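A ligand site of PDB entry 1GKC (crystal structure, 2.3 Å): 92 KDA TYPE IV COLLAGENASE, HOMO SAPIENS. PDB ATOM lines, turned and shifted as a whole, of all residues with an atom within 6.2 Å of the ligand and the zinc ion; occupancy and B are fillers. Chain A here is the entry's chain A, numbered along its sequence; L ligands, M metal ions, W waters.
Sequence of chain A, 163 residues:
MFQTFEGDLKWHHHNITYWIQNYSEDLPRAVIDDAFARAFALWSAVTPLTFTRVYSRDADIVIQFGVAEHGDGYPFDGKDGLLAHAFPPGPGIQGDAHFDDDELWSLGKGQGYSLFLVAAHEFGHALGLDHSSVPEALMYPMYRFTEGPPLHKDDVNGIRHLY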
ATOM      1  N   ASP A  80      30.468   4.539 -34.874  1.00  0.00           N
ATOM      2  CA  ASP A  80      31.486   4.053 -33.935  1.00  0.00           C
ATOM      3  C   ASP A  80      31.660   4.857 -32.651  1.00  0.00           C
ATOM      4  O   ASP A  80      30.915   5.787 -32.386  1.00  0.00           O
ATOM      5  CB  ASP A  80      32.833   3.929 -34.633  1.00  0.00           C
ATOM      6  CG  ASP A  80      32.803   2.886 -35.731  1.00  0.00           C
ATOM      7  OD1 ASP A  80      32.641   1.697 -35.404  1.00  0.00           O
ATOM      8  OD2 ASP A  80      32.942   3.274 -36.910  1.00  0.00           O
ATOM      9  N   GLY A  81      32.668   4.493 -31.875  1.00  0.00           N
ATOM     10  CA  GLY A  81      32.910   5.181 -30.628  1.00  0.00           C
ATOM     11  C   GLY A  81      32.002   4.599 -29.565  1.00  0.00           C
ATOM     12  O   GLY A  81      32.060   3.408 -29.279  1.00  0.00           O
ATOM     13  N   LEU A  82      31.135   5.445 -28.988  1.00  0.00           N
ATOM     14  CA  LEU A  82      30.196   5.005 -27.970  1.00  0.00           C
ATOM     15  C   LEU A  82      29.061   4.259 -28.688  1.00  0.00           C
ATOM     16  O   LEU A  82      28.451   4.818 -29.589  1.00  0.00           O
ATOM     17  CB  LEU A  82      29.626   6.215 -27.227  1.00  0.00           C
ATOM     18  CG  LEU A  82      28.725   5.890 -26.030  1.00  0.00           C
ATOM     19  CD1 LEU A  82      29.559   5.236 -24.930  1.00  0.00           C
ATOM     20  CD2 LEU A  82      28.064   7.171 -25.520  1.00  0.00           C
ATOM     21  N   LEU A  83      28.778   3.026 -28.294  1.00  0.00           N
ATOM     22  CA  LEU A  83      27.727   2.255 -28.952  1.00  0.00           C
ATOM     23  C   LEU A  83      26.352   2.424 -28.316  1.00  0.00           C
ATOM     24  O   LEU A  83      25.321   2.354 -29.000  1.00  0.00           O
ATOM     25  CB  LEU A  83      28.107   0.774 -28.976  1.00  0.00           C
ATOM     26  CG  LEU A  83      29.503   0.425 -29.515  1.00  0.00           C
ATOM     27  CD1 LEU A  83      29.716  -1.085 -29.445  1.00  0.00           C
ATOM     28  CD2 LEU A  83      29.664   0.920 -30.942  1.00  0.00           C
ATOM     29  N   ALA A  84      26.345   2.642 -27.013  1.00  0.00           N
ATOM     30  CA  ALA A  84      25.102   2.788 -26.263  1.00  0.00           C
ATOM     31  C   ALA A  84      25.447   3.163 -24.831  1.00  0.00           C
ATOM     32  O   ALA A  84      26.614   3.310 -24.475  1.00  0.00           O
ATOM     33  CB  ALA A  84      24.340   1.475 -26.286  1.00  0.00           C
ATOM     34  N   HIS A  85      24.413   3.354 -24.020  1.00  0.00           N
ATOM     35  CA  HIS A  85      24.600   3.660 -22.618  1.00  0.00           C
ATOM     36  C   HIS A  85      23.307   3.379 -21.861  1.00  0.00           C
ATOM     37  O   HIS A  85      22.223   3.470 -22.431  1.00  0.00           O
ATOM     38  CB  HIS A  85      25.098   5.109 -22.411  1.00  0.00           C
ATOM     39  CG  HIS A  85      24.180   6.187 -22.901  1.00  0.00           C
ATOM     40  ND1 HIS A  85      24.642   7.321 -23.532  1.00  0.00           N
ATOM     41  CD2 HIS A  85      22.837   6.335 -22.794  1.00  0.00           C
ATOM     42  CE1 HIS A  85      23.628   8.128 -23.780  1.00  0.00           C
ATOM     43  NE2 HIS A  85      22.524   7.548 -23.352  1.00  0.00           N
ATOM     44  N   ALA A  86      23.438   2.998 -20.594  1.00  0.00           N
ATOM     45  CA  ALA A  86      22.274   2.689 -19.754  1.00  0.00           C
ATOM     46  C   ALA A  86      22.408   3.362 -18.391  1.00  0.00           C
ATOM     47  O   ALA A  86      23.504   3.750 -18.002  1.00  0.00           O
ATOM     48  CB  ALA A  86      22.132   1.179 -19.580  1.00  0.00           C
ATOM     49  N   GLU A 103      25.027   3.437 -35.604  1.00  0.00           N
ATOM     50  CA  GLU A 103      25.847   2.247 -35.705  1.00  0.00           C
ATOM     51  C   GLU A 103      25.091   1.276 -36.576  1.00  0.00           C
ATOM     52  O   GLU A 103      23.878   1.357 -36.696  1.00  0.00           O
ATOM     53  CB  GLU A 103      26.037   1.618 -34.324  1.00  0.00           C
ATOM     54  CG  GLU A 103      26.546   2.566 -33.263  1.00  0.00           C
ATOM     55  CD  GLU A 103      27.989   2.929 -33.473  1.00  0.00           C
ATOM     56  OE1 GLU A 103      28.450   2.941 -34.641  1.00  0.00           O
ATOM     57  OE2 GLU A 103      28.678   3.209 -32.483  1.00  0.00           O
ATOM     58  N   TYR A 113      27.712  -4.350 -35.318  1.00  0.00           N
ATOM     59  CA  TYR A 113      27.813  -4.747 -33.916  1.00  0.00           C
ATOM     60  C   TYR A 113      26.639  -5.640 -33.506  1.00  0.00           C
ATOM     61  O   TYR A 113      25.515  -5.429 -33.949  1.00  0.00           O
ATOM     62  CB  TYR A 113      27.848  -3.502 -33.032  1.00  0.00           C
ATOM     63  CG  TYR A 113      29.049  -2.623 -33.251  1.00  0.00           C
ATOM     64  CD1 TYR A 113      30.278  -2.930 -32.671  1.00  0.00           C
ATOM     65  CD2 TYR A 113      28.958  -1.450 -34.020  1.00  0.00           C
ATOM     66  CE1 TYR A 113      31.395  -2.107 -32.842  1.00  0.00           C
ATOM     67  CE2 TYR A 113      30.070  -0.619 -34.205  1.00  0.00           C
ATOM     68  CZ  TYR A 113      31.281  -0.950 -33.612  1.00  0.00           C
ATOM     69  OH  TYR A 113      32.375  -0.132 -33.777  1.00  0.00           O
ATOM     70  N   LEU A 117      24.625  -8.909 -27.923  1.00  0.00           N
ATOM     71  CA  LEU A 117      25.700  -8.774 -26.958  1.00  0.00           C
ATOM     72  C   LEU A 117      25.757  -7.398 -26.307  1.00  0.00           C
ATOM     73  O   LEU A 117      26.064  -7.280 -25.122  1.00  0.00           O
ATOM     74  CB  LEU A 117      27.053  -9.078 -27.615  1.00  0.00           C
ATOM     75  CG  LEU A 117      27.337 -10.535 -27.990  1.00  0.00           C
ATOM     76  CD1 LEU A 117      28.722 -10.655 -28.636  1.00  0.00           C
ATOM     77  CD2 LEU A 117      27.238 -11.406 -26.743  1.00  0.00           C
ATOM     78  N   VAL A 118      25.482  -6.345 -27.078  1.00  0.00           N
ATOM     79  CA  VAL A 118      25.521  -4.999 -26.529  1.00  0.00           C
ATOM     80  C   VAL A 118      24.337  -4.779 -25.583  1.00  0.00           C
ATOM     81  O   VAL A 118      24.466  -4.110 -24.572  1.00  0.00           O
ATOM     82  CB  VAL A 118      25.515  -3.930 -27.643  1.00  0.00           C
ATOM     83  CG1 VAL A 118      25.420  -2.523 -27.038  1.00  0.00           C
ATOM     84  CG2 VAL A 118      26.800  -4.055 -28.494  1.00  0.00           C
ATOM     85  N   HIS A 121      24.983  -6.231 -22.191  1.00  0.00           N
ATOM     86  CA  HIS A 121      25.883  -5.367 -21.436  1.00  0.00           C
ATOM     87  C   HIS A 121      25.114  -4.199 -20.826  1.00  0.00           C
ATOM     88  O   HIS A 121      25.247  -3.911 -19.646  1.00  0.00           O
ATOM     89  CB  HIS A 121      26.975  -4.831 -22.356  1.00  0.00           C
ATOM     90  CG  HIS A 121      27.997  -3.975 -21.665  1.00  0.00           C
ATOM     91  ND1 HIS A 121      29.134  -4.492 -21.082  1.00  0.00           N
ATOM     92  CD2 HIS A 121      28.050  -2.635 -21.463  1.00  0.00           C
ATOM     93  CE1 HIS A 121      29.846  -3.507 -20.566  1.00  0.00           C
ATOM     94  NE2 HIS A 121      29.203  -2.371 -20.780  1.00  0.00           N
ATOM     95  N   GLU A 122      24.308  -3.530 -21.646  1.00  0.00           N
ATOM     96  CA  GLU A 122      23.522  -2.389 -21.172  1.00  0.00           C
ATOM     97  C   GLU A 122      22.550  -2.815 -20.071  1.00  0.00           C
ATOM     98  O   GLU A 122      22.387  -2.102 -19.080  1.00  0.00           O
ATOM     99  CB  GLU A 122      22.732  -1.745 -22.321  1.00  0.00           C
ATOM    100  CG  GLU A 122      23.585  -1.154 -23.443  1.00  0.00           C
ATOM    101  CD  GLU A 122      24.893  -0.546 -22.954  1.00  0.00           C
ATOM    102  OE1 GLU A 122      24.863   0.238 -21.993  1.00  0.00           O
ATOM    103  OE2 GLU A 122      25.940  -0.856 -23.537  1.00  0.00           O
ATOM    104  N   HIS A 125      24.097  -2.912 -16.719  1.00  0.00           N
ATOM    105  CA  HIS A 125      24.119  -1.610 -16.056  1.00  0.00           C
ATOM    106  C   HIS A 125      22.755  -1.286 -15.460  1.00  0.00           C
ATOM    107  O   HIS A 125      22.642  -0.871 -14.311  1.00  0.00           O
ATOM    108  CB  HIS A 125      24.490  -0.505 -17.044  1.00  0.00           C
ATOM    109  CG  HIS A 125      25.939  -0.457 -17.390  1.00  0.00           C
ATOM    110  ND1 HIS A 125      26.933  -0.537 -16.429  1.00  0.00           N
ATOM    111  CD2 HIS A 125      26.567  -0.324 -18.571  1.00  0.00           C
ATOM    112  CE1 HIS A 125      28.110  -0.457 -17.022  1.00  0.00           C
ATOM    113  NE2 HIS A 125      27.911  -0.331 -18.321  1.00  0.00           N
ATOM    114  N   HIS A 131      31.331  -1.586 -14.444  1.00  0.00           N
ATOM    115  CA  HIS A 131      32.281  -2.184 -15.378  1.00  0.00           C
ATOM    116  C   HIS A 131      33.219  -3.159 -14.687  1.00  0.00           C
ATOM    117  O   HIS A 131      33.572  -2.970 -13.521  1.00  0.00           O
ATOM    118  CB  HIS A 131      33.072  -1.102 -16.084  1.00  0.00           C
ATOM    119  CG  HIS A 131      32.342  -0.456 -17.219  1.00  0.00           C
ATOM    120  ND1 HIS A 131      32.535   0.853 -17.593  1.00  0.00           N
ATOM    121  CD2 HIS A 131      31.402  -0.955 -18.062  1.00  0.00           C
ATOM    122  CE1 HIS A 131      31.755   1.136 -18.620  1.00  0.00           C
ATOM    123  NE2 HIS A 131      31.053   0.051 -18.925  1.00  0.00           N
ATOM    124  N   LEU A 138      31.613  -9.963 -19.731  1.00  0.00           N
ATOM    125  CA  LEU A 138      30.669  -9.212 -20.543  1.00  0.00           C
ATOM    126  C   LEU A 138      30.632  -7.738 -20.144  1.00  0.00           C
ATOM    127  O   LEU A 138      30.381  -6.870 -20.976  1.00  0.00           O
ATOM    128  CB  LEU A 138      29.263  -9.803 -20.389  1.00  0.00           C
ATOM    129  CG  LEU A 138      28.102  -9.064 -21.071  1.00  0.00           C
ATOM    130  CD1 LEU A 138      28.310  -9.041 -22.560  1.00  0.00           C
ATOM    131  CD2 LEU A 138      26.778  -9.733 -20.726  1.00  0.00           C
ATOM    132  N   MET A 139      30.892  -7.463 -18.865  1.00  0.00           N
ATOM    133  CA  MET A 139      30.861  -6.087 -18.385  1.00  0.00           C
ATOM    134  C   MET A 139      32.150  -5.305 -18.630  1.00  0.00           C
ATOM    135  O   MET A 139      32.307  -4.188 -18.161  1.00  0.00           O
ATOM    136  CB  MET A 139      30.505  -6.039 -16.898  1.00  0.00           C
ATOM    137  CG  MET A 139      29.064  -6.445 -16.601  1.00  0.00           C
ATOM    138  SD  MET A 139      27.792  -5.691 -17.698  1.00  0.00           S
ATOM    139  CE  MET A 139      27.913  -3.976 -17.294  1.00  0.00           C
ATOM    140  N   TYR A 140      33.070  -5.897 -19.381  1.00  0.00           N
ATOM    141  CA  TYR A 140      34.300  -5.196 -19.714  1.00  0.00           C
ATOM    142  C   TYR A 140      33.856  -3.988 -20.549  1.00  0.00           C
ATOM    143  O   TYR A 140      33.039  -4.132 -21.469  1.00  0.00           O
ATOM    144  CB  TYR A 140      35.227  -6.097 -20.528  1.00  0.00           C
ATOM    145  CG  TYR A 140      36.636  -5.573 -20.652  1.00  0.00           C
ATOM    146  CD1 TYR A 140      37.452  -5.454 -19.523  1.00  0.00           C
ATOM    147  CD2 TYR A 140      37.137  -5.176 -21.883  1.00  0.00           C
ATOM    148  CE1 TYR A 140      38.746  -4.955 -19.626  1.00  0.00           C
ATOM    149  CE2 TYR A 140      38.425  -4.668 -22.001  1.00  0.00           C
ATOM    150  CZ  TYR A 140      39.228  -4.567 -20.870  1.00  0.00           C
ATOM    151  OH  TYR A 140      40.506  -4.080 -20.995  1.00  0.00           O
ATOM    152  N   PRO A 141      34.377  -2.795 -20.255  1.00  0.00           N
ATOM    153  CA  PRO A 141      34.043  -1.533 -20.938  1.00  0.00           C
ATOM    154  C   PRO A 141      34.278  -1.425 -22.443  1.00  0.00           C
ATOM    155  O   PRO A 141      33.920  -0.413 -23.053  1.00  0.00           O
ATOM    156  CB  PRO A 141      34.842  -0.495 -20.149  1.00  0.00           C
ATOM    157  CG  PRO A 141      36.043  -1.259 -19.727  1.00  0.00           C
ATOM    158  CD  PRO A 141      35.470  -2.578 -19.275  1.00  0.00           C
ATOM    159  N   MET A 142      34.862  -2.459 -23.040  1.00  0.00           N
ATOM    160  CA  MET A 142      35.162  -2.459 -24.457  1.00  0.00           C
ATOM    161  C   MET A 142      34.388  -3.561 -25.180  1.00  0.00           C
ATOM    162  O   MET A 142      34.212  -4.662 -24.657  1.00  0.00           O
ATOM    163  CB  MET A 142      36.671  -2.677 -24.631  1.00  0.00           C
ATOM    164  CG  MET A 142      37.151  -2.757 -26.057  1.00  0.00           C
ATOM    165  SD  MET A 142      38.875  -3.316 -26.116  1.00  0.00           S
ATOM    166  CE  MET A 142      38.678  -5.042 -26.590  1.00  0.00           C
ATOM    167  N   TYR A 143      33.912  -3.263 -26.381  1.00  0.00           N
ATOM    168  CA  TYR A 143      33.156  -4.253 -27.151  1.00  0.00           C
ATOM    169  C   TYR A 143      34.065  -5.339 -27.738  1.00  0.00           C
ATOM    170  O   TYR A 143      35.130  -5.036 -28.271  1.00  0.00           O
ATOM    171  CB  TYR A 143      32.415  -3.590 -28.315  1.00  0.00           C
ATOM    172  CG  TYR A 143      31.709  -4.580 -29.222  1.00  0.00           C
ATOM    173  CD1 TYR A 143      30.428  -5.038 -28.925  1.00  0.00           C
ATOM    174  CD2 TYR A 143      32.336  -5.076 -30.370  1.00  0.00           C
ATOM    175  CE1 TYR A 143      29.780  -5.968 -29.749  1.00  0.00           C
ATOM    176  CE2 TYR A 143      31.699  -5.998 -31.193  1.00  0.00           C
ATOM    177  CZ  TYR A 143      30.425  -6.444 -30.876  1.00  0.00           C
ATOM    178  OH  TYR A 143      29.788  -7.353 -31.692  1.00  0.00           O
ATOM    179  N   ARG A 144      33.628  -6.590 -27.654  1.00  0.00           N
ATOM    180  CA  ARG A 144      34.383  -7.693 -28.221  1.00  0.00           C
ATOM    181  C   ARG A 144      33.424  -8.817 -28.600  1.00  0.00           C
ATOM    182  O   ARG A 144      32.755  -9.390 -27.747  1.00  0.00           O
ATOM    183  CB  ARG A 144      35.461  -8.206 -27.249  1.00  0.00           C
ATOM    184  CG  ARG A 144      34.935  -9.046 -26.106  1.00  0.00           C
ATOM    185  CD  ARG A 144      36.069  -9.660 -25.305  1.00  0.00           C
ATOM    186  NE  ARG A 144      35.569 -10.598 -24.300  1.00  0.00           N
ATOM    187  CZ  ARG A 144      34.920 -11.723 -24.591  1.00  0.00           C
ATOM    188  NH1 ARG A 144      34.691 -12.053 -25.858  1.00  0.00           N
ATOM    189  NH2 ARG A 144      34.481 -12.514 -23.620  1.00  0.00           N
HETATM  190  C1  LIG L   1      31.244   1.243 -25.629  1.00  0.00           C
HETATM  191  N1  LIG L   1      29.231   1.383 -22.372  1.00  0.00           N
HETATM  192  O1  LIG L   1      30.501   1.847 -26.447  1.00  0.00           O
HETATM  193  C2  LIG L   1      33.558   0.478 -28.001  1.00  0.00           C
HETATM  194  N2  LIG L   1      32.577   1.125 -25.799  1.00  0.00           N
HETATM  195  O2  LIG L   1      33.940  -0.638 -27.602  1.00  0.00           O
HETATM  196  N3  LIG L   1      33.288   0.776 -29.301  1.00  0.00           N
HETATM  197  C3  LIG L   1      30.624   0.609 -24.352  1.00  0.00           C
HETATM  198  C4  LIG L   1      29.615  -0.570 -24.697  1.00  0.00           C
HETATM  199  C5  LIG L   1      30.140  -1.853 -25.389  1.00  0.00           C
HETATM  200  C6  LIG L   1      27.923   1.190 -22.218  1.00  0.00           C
HETATM  201  O3  LIG L   1      27.409   0.850 -21.208  1.00  0.00           O
HETATM  202  C7  LIG L   1      29.857   1.779 -23.636  1.00  0.00           C
HETATM  203  O4  LIG L   1      30.011   1.198 -21.372  1.00  0.00           O
HETATM  204  C8  LIG L   1      33.329   1.691 -26.982  1.00  0.00           C
HETATM  205  C9  LIG L   1      34.689   2.447 -26.531  1.00  0.00           C
HETATM  206  C10 LIG L   1      31.103  -2.614 -24.463  1.00  0.00           C
HETATM  207  C11 LIG L   1      28.971  -2.805 -25.611  1.00  0.00           C
HETATM  208  C12 LIG L   1      35.477   3.039 -27.755  1.00  0.00           C
HETATM  209  C13 LIG L   1      34.369   3.607 -25.552  1.00  0.00           C
HETATM  210  C14 LIG L   1      35.709   1.511 -25.778  1.00  0.00           C
HETATM  211  C15 LIG L   1      33.415  -0.179 -30.426  1.00  0.00           C
HETATM  212 ZN    ZN M   1      29.214  -0.255 -20.129  1.00  0.00          ZN
HETATM  213  O   HOH W   1      26.172   3.070 -19.627  1.00  0.00           O
HETATM  214  O   HOH W   2      32.844   1.790 -21.822  1.00  0.00           O
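A ring nitrogen (ND1) of His 121 lies within hydrogen-bond range of the backbone carbonyl oxygen of Leu 138, at 2.7 Å. The backbone NH (N) of Ala 86 is in hydrogen-bond range of the side-chain carboxylate (OE1) of Glu 122. The side-chain carboxylate (OD1) of Asp 80 sits at hydrogen-bond distance from the side-chain hydroxyl (OH) of Tyr 113, 2.5 Å away.
Merely in contact with the ligand: Ala 84, Met 142, Tyr 113, Leu 82, Val 118 and Tyr 140. Hydrophobic or aromatic side chains that line the ligand: Leu 82, Leu 83, Tyr 113, Val 118, His 121, His 125, His 131 and Tyr 143. 14 residues have an atom within 4 Å of the ligand: Gly 81, Leu 82, Leu 83, Ala 84, Tyr 113, Val 118, His 121, Glu 122, His 125, His 131, Tyr 140, Pro 141, Met 142 and Tyr 143.
O4 of the ligand is bound to the zinc ion (2.1 Å). The zinc ion is bound by NE2 of His 121. NE2 of His 131 binds the zinc ion (2.2 Å). The zinc ion is bound by a ring nitrogen (NE2) of His 125, 2.2 Å away. The zinc ion is bound by O3 of the ligand, 2.4 Å away. The zinc ion has five donor atoms within binding distance.
O3 of the ligand sits close to OE1 of Glu 122, 2.7 Å away. N of Leu 83 is in hydrogen-bond range of O1 of the ligand, 2.8 Å away. An oxygen (O2) of the ligand sits at hydrogen-bond distance from the backbone NH (N) of Tyr 143 (2.9 Å). N3 of the ligand sits at hydrogen-bond distance from O of Gly 81, 2.9 Å away. O of Pro 141 is in hydrogen-bond range of N2 of the ligand, 3.4 Å away.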
